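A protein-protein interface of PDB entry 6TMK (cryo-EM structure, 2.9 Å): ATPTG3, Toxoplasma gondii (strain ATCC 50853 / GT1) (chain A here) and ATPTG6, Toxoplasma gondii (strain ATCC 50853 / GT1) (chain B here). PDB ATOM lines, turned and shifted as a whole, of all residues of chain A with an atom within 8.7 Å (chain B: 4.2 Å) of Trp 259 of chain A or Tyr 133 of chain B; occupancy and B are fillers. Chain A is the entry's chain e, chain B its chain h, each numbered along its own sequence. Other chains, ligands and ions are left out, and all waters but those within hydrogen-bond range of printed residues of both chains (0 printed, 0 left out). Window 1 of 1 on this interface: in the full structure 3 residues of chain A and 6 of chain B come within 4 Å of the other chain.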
ATOM      1  N   GLY A 254      18.414  27.522 -33.925  1.00  0.00           N
ATOM      2  CA  GLY A 254      19.163  28.178 -32.878  1.00  0.00           C
ATOM      3  C   GLY A 254      18.640  27.965 -31.483  1.00  0.00           C
ATOM      4  O   GLY A 254      18.974  28.742 -30.586  1.00  0.00           O
ATOM      5  N   VAL A 256      19.073  25.120 -29.705  1.00  0.00           N
ATOM      6  CA  VAL A 256      19.738  23.951 -29.147  1.00  0.00           C
ATOM      7  C   VAL A 256      21.239  24.115 -29.332  1.00  0.00           C
ATOM      8  O   VAL A 256      21.709  24.516 -30.400  1.00  0.00           O
ATOM      9  CB  VAL A 256      19.221  22.659 -29.810  1.00  0.00           C
ATOM     10  CG1 VAL A 256      20.172  21.528 -29.581  1.00  0.00           C
ATOM     11  CG2 VAL A 256      17.862  22.309 -29.273  1.00  0.00           C
ATOM     12  N   SER A 257      21.986  23.802 -28.279  1.00  0.00           N
ATOM     13  CA  SER A 257      23.448  23.802 -28.289  1.00  0.00           C
ATOM     14  C   SER A 257      23.899  22.507 -27.633  1.00  0.00           C
ATOM     15  O   SER A 257      24.205  22.483 -26.434  1.00  0.00           O
ATOM     16  CB  SER A 257      24.015  25.029 -27.579  1.00  0.00           C
ATOM     17  OG  SER A 257      23.726  26.212 -28.301  1.00  0.00           O
ATOM     18  N   PRO A 258      23.957  21.405 -28.385  1.00  0.00           N
ATOM     19  CA  PRO A 258      24.179  20.110 -27.731  1.00  0.00           C
ATOM     20  C   PRO A 258      25.562  19.954 -27.138  1.00  0.00           C
ATOM     21  O   PRO A 258      25.719  19.195 -26.175  1.00  0.00           O
ATOM     22  CB  PRO A 258      23.946  19.102 -28.866  1.00  0.00           C
ATOM     23  CG  PRO A 258      23.234  19.863 -29.918  1.00  0.00           C
ATOM     24  CD  PRO A 258      23.775  21.239 -29.831  1.00  0.00           C
ATOM     25  N   TRP A 259      26.575  20.627 -27.683  1.00  0.00           N
ATOM     26  CA  TRP A 259      27.908  20.509 -27.113  1.00  0.00           C
ATOM     27  C   TRP A 259      27.951  21.037 -25.688  1.00  0.00           C
ATOM     28  O   TRP A 259      28.679  20.500 -24.848  1.00  0.00           O
ATOM     29  CB  TRP A 259      28.920  21.251 -27.985  1.00  0.00           C
ATOM     30  CG  TRP A 259      28.662  22.712 -28.123  1.00  0.00           C
ATOM     31  CD1 TRP A 259      29.136  23.703 -27.325  1.00  0.00           C
ATOM     32  CD2 TRP A 259      27.878  23.352 -29.132  1.00  0.00           C
ATOM     33  NE1 TRP A 259      28.691  24.921 -27.765  1.00  0.00           N
ATOM     34  CE2 TRP A 259      27.916  24.731 -28.877  1.00  0.00           C
ATOM     35  CE3 TRP A 259      27.148  22.890 -30.224  1.00  0.00           C
ATOM     36  CZ2 TRP A 259      27.254  25.652 -29.671  1.00  0.00           C
ATOM     37  CZ3 TRP A 259      26.490  23.802 -31.011  1.00  0.00           C
ATOM     38  CH2 TRP A 259      26.544  25.169 -30.732  1.00  0.00           C
ATOM     39  N   GLU A 260      27.161  22.064 -25.392  1.00  0.00           N
ATOM     40  CA  GLU A 260      27.133  22.625 -24.052  1.00  0.00           C
ATOM     41  C   GLU A 260      26.416  21.696 -23.087  1.00  0.00           C
ATOM     42  O   GLU A 260      25.324  21.199 -23.376  1.00  0.00           O
ATOM     43  CB  GLU A 260      26.439  23.983 -24.072  1.00  0.00           C
ATOM     44  CG  GLU A 260      27.018  24.955 -25.079  1.00  0.00           C
ATOM     45  CD  GLU A 260      26.406  26.335 -24.978  1.00  0.00           C
ATOM     46  OE1 GLU A 260      26.909  27.257 -25.652  1.00  0.00           O
ATOM     47  OE2 GLU A 260      25.417  26.499 -24.234  1.00  0.00           O
ATOM     48  N   GLU A 261      27.037  21.453 -21.940  1.00  0.00           N
ATOM     49  CA  GLU A 261      26.347  20.781 -20.854  1.00  0.00           C
ATOM     50  C   GLU A 261      25.365  21.763 -20.224  1.00  0.00           C
ATOM     51  O   GLU A 261      25.761  22.844 -19.777  1.00  0.00           O
ATOM     52  CB  GLU A 261      27.352  20.263 -19.830  1.00  0.00           C
ATOM     53  CG  GLU A 261      26.729  19.498 -18.695  1.00  0.00           C
ATOM     54  CD  GLU A 261      26.492  18.047 -19.048  1.00  0.00           C
ATOM     55  OE1 GLU A 261      27.486  17.313 -19.223  1.00  0.00           O
ATOM     56  OE2 GLU A 261      25.315  17.638 -19.152  1.00  0.00           O
ATOM     57  N   THR A 262      24.090  21.388 -20.185  1.00  0.00           N
ATOM     58  CA  THR A 262      23.033  22.286 -19.744  1.00  0.00           C
ATOM     59  C   THR A 262      22.563  22.020 -18.325  1.00  0.00           C
ATOM     60  O   THR A 262      21.914  22.888 -17.732  1.00  0.00           O
ATOM     61  CB  THR A 262      21.837  22.198 -20.693  1.00  0.00           C
ATOM     62  OG1 THR A 262      21.601  20.830 -21.041  1.00  0.00           O
ATOM     63  CG2 THR A 262      22.101  22.992 -21.951  1.00  0.00           C
ATOM     64  N   PRO B 116      35.699  13.715 -20.332  1.00  0.00           N
ATOM     65  CA  PRO B 116      36.683  14.795 -20.376  1.00  0.00           C
ATOM     66  C   PRO B 116      36.341  15.984 -19.490  1.00  0.00           C
ATOM     67  O   PRO B 116      35.191  16.225 -19.119  1.00  0.00           O
ATOM     68  CB  PRO B 116      36.653  15.206 -21.849  1.00  0.00           C
ATOM     69  CG  PRO B 116      35.255  15.015 -22.230  1.00  0.00           C
ATOM     70  CD  PRO B 116      34.736  13.839 -21.440  1.00  0.00           C
ATOM     71  N   PHE B 118      37.378  19.699 -20.416  1.00  0.00           N
ATOM     72  CA  PHE B 118      37.983  20.456 -21.498  1.00  0.00           C
ATOM     73  C   PHE B 118      38.600  21.743 -20.972  1.00  0.00           C
ATOM     74  O   PHE B 118      37.988  22.459 -20.174  1.00  0.00           O
ATOM     75  CB  PHE B 118      36.931  20.782 -22.553  1.00  0.00           C
ATOM     76  CG  PHE B 118      36.577  19.636 -23.440  1.00  0.00           C
ATOM     77  CD1 PHE B 118      37.482  19.140 -24.349  1.00  0.00           C
ATOM     78  CD2 PHE B 118      35.329  19.060 -23.373  1.00  0.00           C
ATOM     79  CE1 PHE B 118      37.148  18.097 -25.166  1.00  0.00           C
ATOM     80  CE2 PHE B 118      34.997  18.016 -24.190  1.00  0.00           C
ATOM     81  CZ  PHE B 118      35.907  17.535 -25.087  1.00  0.00           C
ATOM     82  N   ASN B 121      36.452  25.951 -24.595  1.00  0.00           N
ATOM     83  CA  ASN B 121      35.159  25.671 -25.200  1.00  0.00           C
ATOM     84  C   ASN B 121      35.289  25.224 -26.650  1.00  0.00           C
ATOM     85  O   ASN B 121      34.449  24.460 -27.141  1.00  0.00           O
ATOM     86  CB  ASN B 121      34.269  26.905 -25.101  1.00  0.00           C
ATOM     87  CG  ASN B 121      32.887  26.672 -25.666  1.00  0.00           C
ATOM     88  OD1 ASN B 121      32.301  25.604 -25.494  1.00  0.00           O
ATOM     89  ND2 ASN B 121      32.360  27.672 -26.354  1.00  0.00           N
ATOM     90  N   ARG B 124      35.723  21.446 -26.973  1.00  0.00           N
ATOM     91  CA  ARG B 124      34.407  20.836 -26.862  1.00  0.00           C
ATOM     92  C   ARG B 124      33.654  20.932 -28.180  1.00  0.00           C
ATOM     93  O   ARG B 124      33.103  19.941 -28.680  1.00  0.00           O
ATOM     94  CB  ARG B 124      33.647  21.543 -25.746  1.00  0.00           C
ATOM     95  CG  ARG B 124      32.406  20.872 -25.247  1.00  0.00           C
ATOM     96  CD  ARG B 124      31.711  21.775 -24.252  1.00  0.00           C
ATOM     97  NE  ARG B 124      32.425  21.842 -22.986  1.00  0.00           N
ATOM     98  CZ  ARG B 124      32.270  20.980 -21.989  1.00  0.00           C
ATOM     99  NH1 ARG B 124      31.421  19.971 -22.101  1.00  0.00           N
ATOM    100  NH2 ARG B 124      32.971  21.128 -20.878  1.00  0.00           N
ATOM    101  N   LEU B 125      33.621  22.134 -28.752  1.00  0.00           N
ATOM    102  CA  LEU B 125      32.956  22.348 -30.029  1.00  0.00           C
ATOM    103  C   LEU B 125      33.505  21.426 -31.105  1.00  0.00           C
ATOM    104  O   LEU B 125      32.744  20.808 -31.850  1.00  0.00           O
ATOM    105  CB  LEU B 125      33.119  23.803 -30.446  1.00  0.00           C
ATOM    106  CG  LEU B 125      32.041  24.757 -29.978  1.00  0.00           C
ATOM    107  CD1 LEU B 125      32.556  26.167 -30.056  1.00  0.00           C
ATOM    108  CD2 LEU B 125      30.833  24.573 -30.862  1.00  0.00           C
ATOM    109  N   ALA B 127      35.257  18.589 -30.878  1.00  0.00           N
ATOM    110  CA  ALA B 127      34.956  17.190 -30.616  1.00  0.00           C
ATOM    111  C   ALA B 127      33.521  16.860 -30.997  1.00  0.00           C
ATOM    112  O   ALA B 127      33.258  15.855 -31.670  1.00  0.00           O
ATOM    113  CB  ALA B 127      35.209  16.878 -29.148  1.00  0.00           C
ATOM    114  N   TYR B 128      32.575  17.705 -30.586  1.00  0.00           N
ATOM    115  CA  TYR B 128      31.190  17.488 -30.976  1.00  0.00           C
ATOM    116  C   TYR B 128      31.027  17.535 -32.487  1.00  0.00           C
ATOM    117  O   TYR B 128      30.348  16.687 -33.077  1.00  0.00           O
ATOM    118  CB  TYR B 128      30.294  18.533 -30.322  1.00  0.00           C
ATOM    119  CG  TYR B 128      28.869  18.463 -30.802  1.00  0.00           C
ATOM    120  CD1 TYR B 128      28.029  17.452 -30.386  1.00  0.00           C
ATOM    121  CD2 TYR B 128      28.378  19.387 -31.706  1.00  0.00           C
ATOM    122  CE1 TYR B 128      26.740  17.376 -30.834  1.00  0.00           C
ATOM    123  CE2 TYR B 128      27.094  19.315 -32.159  1.00  0.00           C
ATOM    124  CZ  TYR B 128      26.277  18.306 -31.724  1.00  0.00           C
ATOM    125  OH  TYR B 128      24.983  18.232 -32.179  1.00  0.00           O
ATOM    126  N   GLY B 131      32.111  14.387 -33.975  1.00  0.00           N
ATOM    127  CA  GLY B 131      31.392  13.208 -33.560  1.00  0.00           C
ATOM    128  C   GLY B 131      32.097  12.393 -32.513  1.00  0.00           C
ATOM    129  O   GLY B 131      31.983  11.164 -32.515  1.00  0.00           O
ATOM    130  N   LEU B 132      32.821  13.043 -31.609  1.00  0.00           N
ATOM    131  CA  LEU B 132      33.624  12.359 -30.614  1.00  0.00           C
ATOM    132  C   LEU B 132      33.246  12.755 -29.199  1.00  0.00           C
ATOM    133  O   LEU B 132      33.947  12.377 -28.256  1.00  0.00           O
ATOM    134  CB  LEU B 132      35.100  12.651 -30.870  1.00  0.00           C
ATOM    135  CG  LEU B 132      35.631  12.183 -32.219  1.00  0.00           C
ATOM    136  CD1 LEU B 132      36.757  13.061 -32.678  1.00  0.00           C
ATOM    137  CD2 LEU B 132      36.083  10.763 -32.151  1.00  0.00           C
ATOM    138  N   TYR B 133      32.154  13.491 -29.023  1.00  0.00           N
ATOM    139  CA  TYR B 133      31.728  13.906 -27.697  1.00  0.00           C
ATOM    140  C   TYR B 133      30.252  14.255 -27.715  1.00  0.00           C
ATOM    141  O   TYR B 133      29.791  14.970 -28.608  1.00  0.00           O
ATOM    142  CB  TYR B 133      32.538  15.104 -27.207  1.00  0.00           C
ATOM    143  CG  TYR B 133      31.947  15.769 -26.002  1.00  0.00           C
ATOM    144  CD1 TYR B 133      32.039  15.189 -24.755  1.00  0.00           C
ATOM    145  CD2 TYR B 133      31.296  16.979 -26.112  1.00  0.00           C
ATOM    146  CE1 TYR B 133      31.501  15.793 -23.654  1.00  0.00           C
ATOM    147  CE2 TYR B 133      30.755  17.590 -25.018  1.00  0.00           C
ATOM    148  CZ  TYR B 133      30.858  16.994 -23.788  1.00  0.00           C
ATOM    149  OH  TYR B 133      30.319  17.599 -22.683  1.00  0.00           O
ATOM    150  N   SER B 134      29.516  13.728 -26.738  1.00  0.00           N
ATOM    151  CA  SER B 134      28.192  14.190 -26.428  1.00  0.00           C
ATOM    152  C   SER B 134      28.071  14.094 -24.910  1.00  0.00           C
ATOM    153  O   SER B 134      28.389  13.040 -24.331  1.00  0.00           O
ATOM    154  CB  SER B 134      27.106  13.369 -27.118  1.00  0.00           C
ATOM    155  OG  SER B 134      26.738  12.240 -26.354  1.00  0.00           O
ATOM    156  N   PRO B 135      27.643  15.160 -24.235  1.00  0.00           N
ATOM    157  CA  PRO B 135      27.516  15.078 -22.774  1.00  0.00           C
ATOM    158  C   PRO B 135      26.480  14.072 -22.330  1.00  0.00           C
ATOM    159  O   PRO B 135      26.665  13.412 -21.298  1.00  0.00           O
ATOM    160  CB  PRO B 135      27.144  16.512 -22.379  1.00  0.00           C
ATOM    161  CG  PRO B 135      26.538  17.093 -23.580  1.00  0.00           C
ATOM    162  CD  PRO B 135      27.201  16.464 -24.750  1.00  0.00           C
ATOM    163  N   PHE B 138      28.744  11.097 -22.148  1.00  0.00           N
ATOM    164  CA  PHE B 138      29.971  11.050 -21.366  1.00  0.00           C
ATOM    165  C   PHE B 138      29.818  11.526 -19.931  1.00  0.00           C
ATOM    166  O   PHE B 138      30.540  11.041 -19.056  1.00  0.00           O
ATOM    167  CB  PHE B 138      31.064  11.858 -22.059  1.00  0.00           C
ATOM    168  CG  PHE B 138      31.658  11.153 -23.222  1.00  0.00           C
ATOM    169  CD1 PHE B 138      32.612  10.181 -23.036  1.00  0.00           C
ATOM    170  CD2 PHE B 138      31.239  11.431 -24.502  1.00  0.00           C
ATOM    171  CE1 PHE B 138      33.147   9.520 -24.099  1.00  0.00           C
ATOM    172  CE2 PHE B 138      31.768  10.773 -25.564  1.00  0.00           C
ATOM    173  CZ  PHE B 138      32.724   9.816 -25.368  1.00  0.00           C
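Among the printed residues, pairs that only touch across the chains: Glu 261 of chain A with Pro 135 of chain B (3.3 Å), Pro 258 of chain A with Tyr 128 of chain B (3.3 Å), Trp 259 of chain A with Arg 124 of chain B (3.3 Å), Pro 258 of chain A with Pro 135 of chain B (3.4 Å), Trp 259 of chain A with Leu 125 of chain B (3.5 Å), Trp 259 of chain A with Tyr 133 of chain B (3.6 Å) and Trp 259 of chain A with Tyr 128 of chain B (3.8 Å).
NH1 of Arg 124 of chain B is in hydrogen-bond range of OH of Tyr 133 of chain B (2.7 Å).
Along chain A the printed residues that touch a printed residue of chain B span positions 258 to 261.
Hydrophobic or aromatic side chains of chain B that line the printed part of chain A: Leu 125, Tyr 128, Tyr 133 and Pro 135.
Of the printed residues of chain B, Glu 261 of chain A touches Pro 135.
Of the printed residues of chain A, Arg 124 of chain B touches Trp 259.
Of the printed residues of chain A, Tyr 128 of chain B touches Pro 258 and Trp 259.
Of chain A, only Trp 259 (3.6 Å) comes within 4 Å of Tyr 133 of chain B.
No residue of chain A comes within 4 Å of Ser 134 of chain B.
Of the printed residues of chain A, Pro 135 of chain B touches Pro 258 and Glu 261.
The nearest residue of chain B that does not touch Trp 259 of chain A is Asn 121 of chain B (4.1 Å).
The nearest residue of chain A that does not touch Tyr 133 of chain B is Glu 261 of chain A (4.5 Å).
The nearest printed residue of chain B that does not touch Glu 261 of chain A is Tyr 133 of chain B (4.5 Å).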
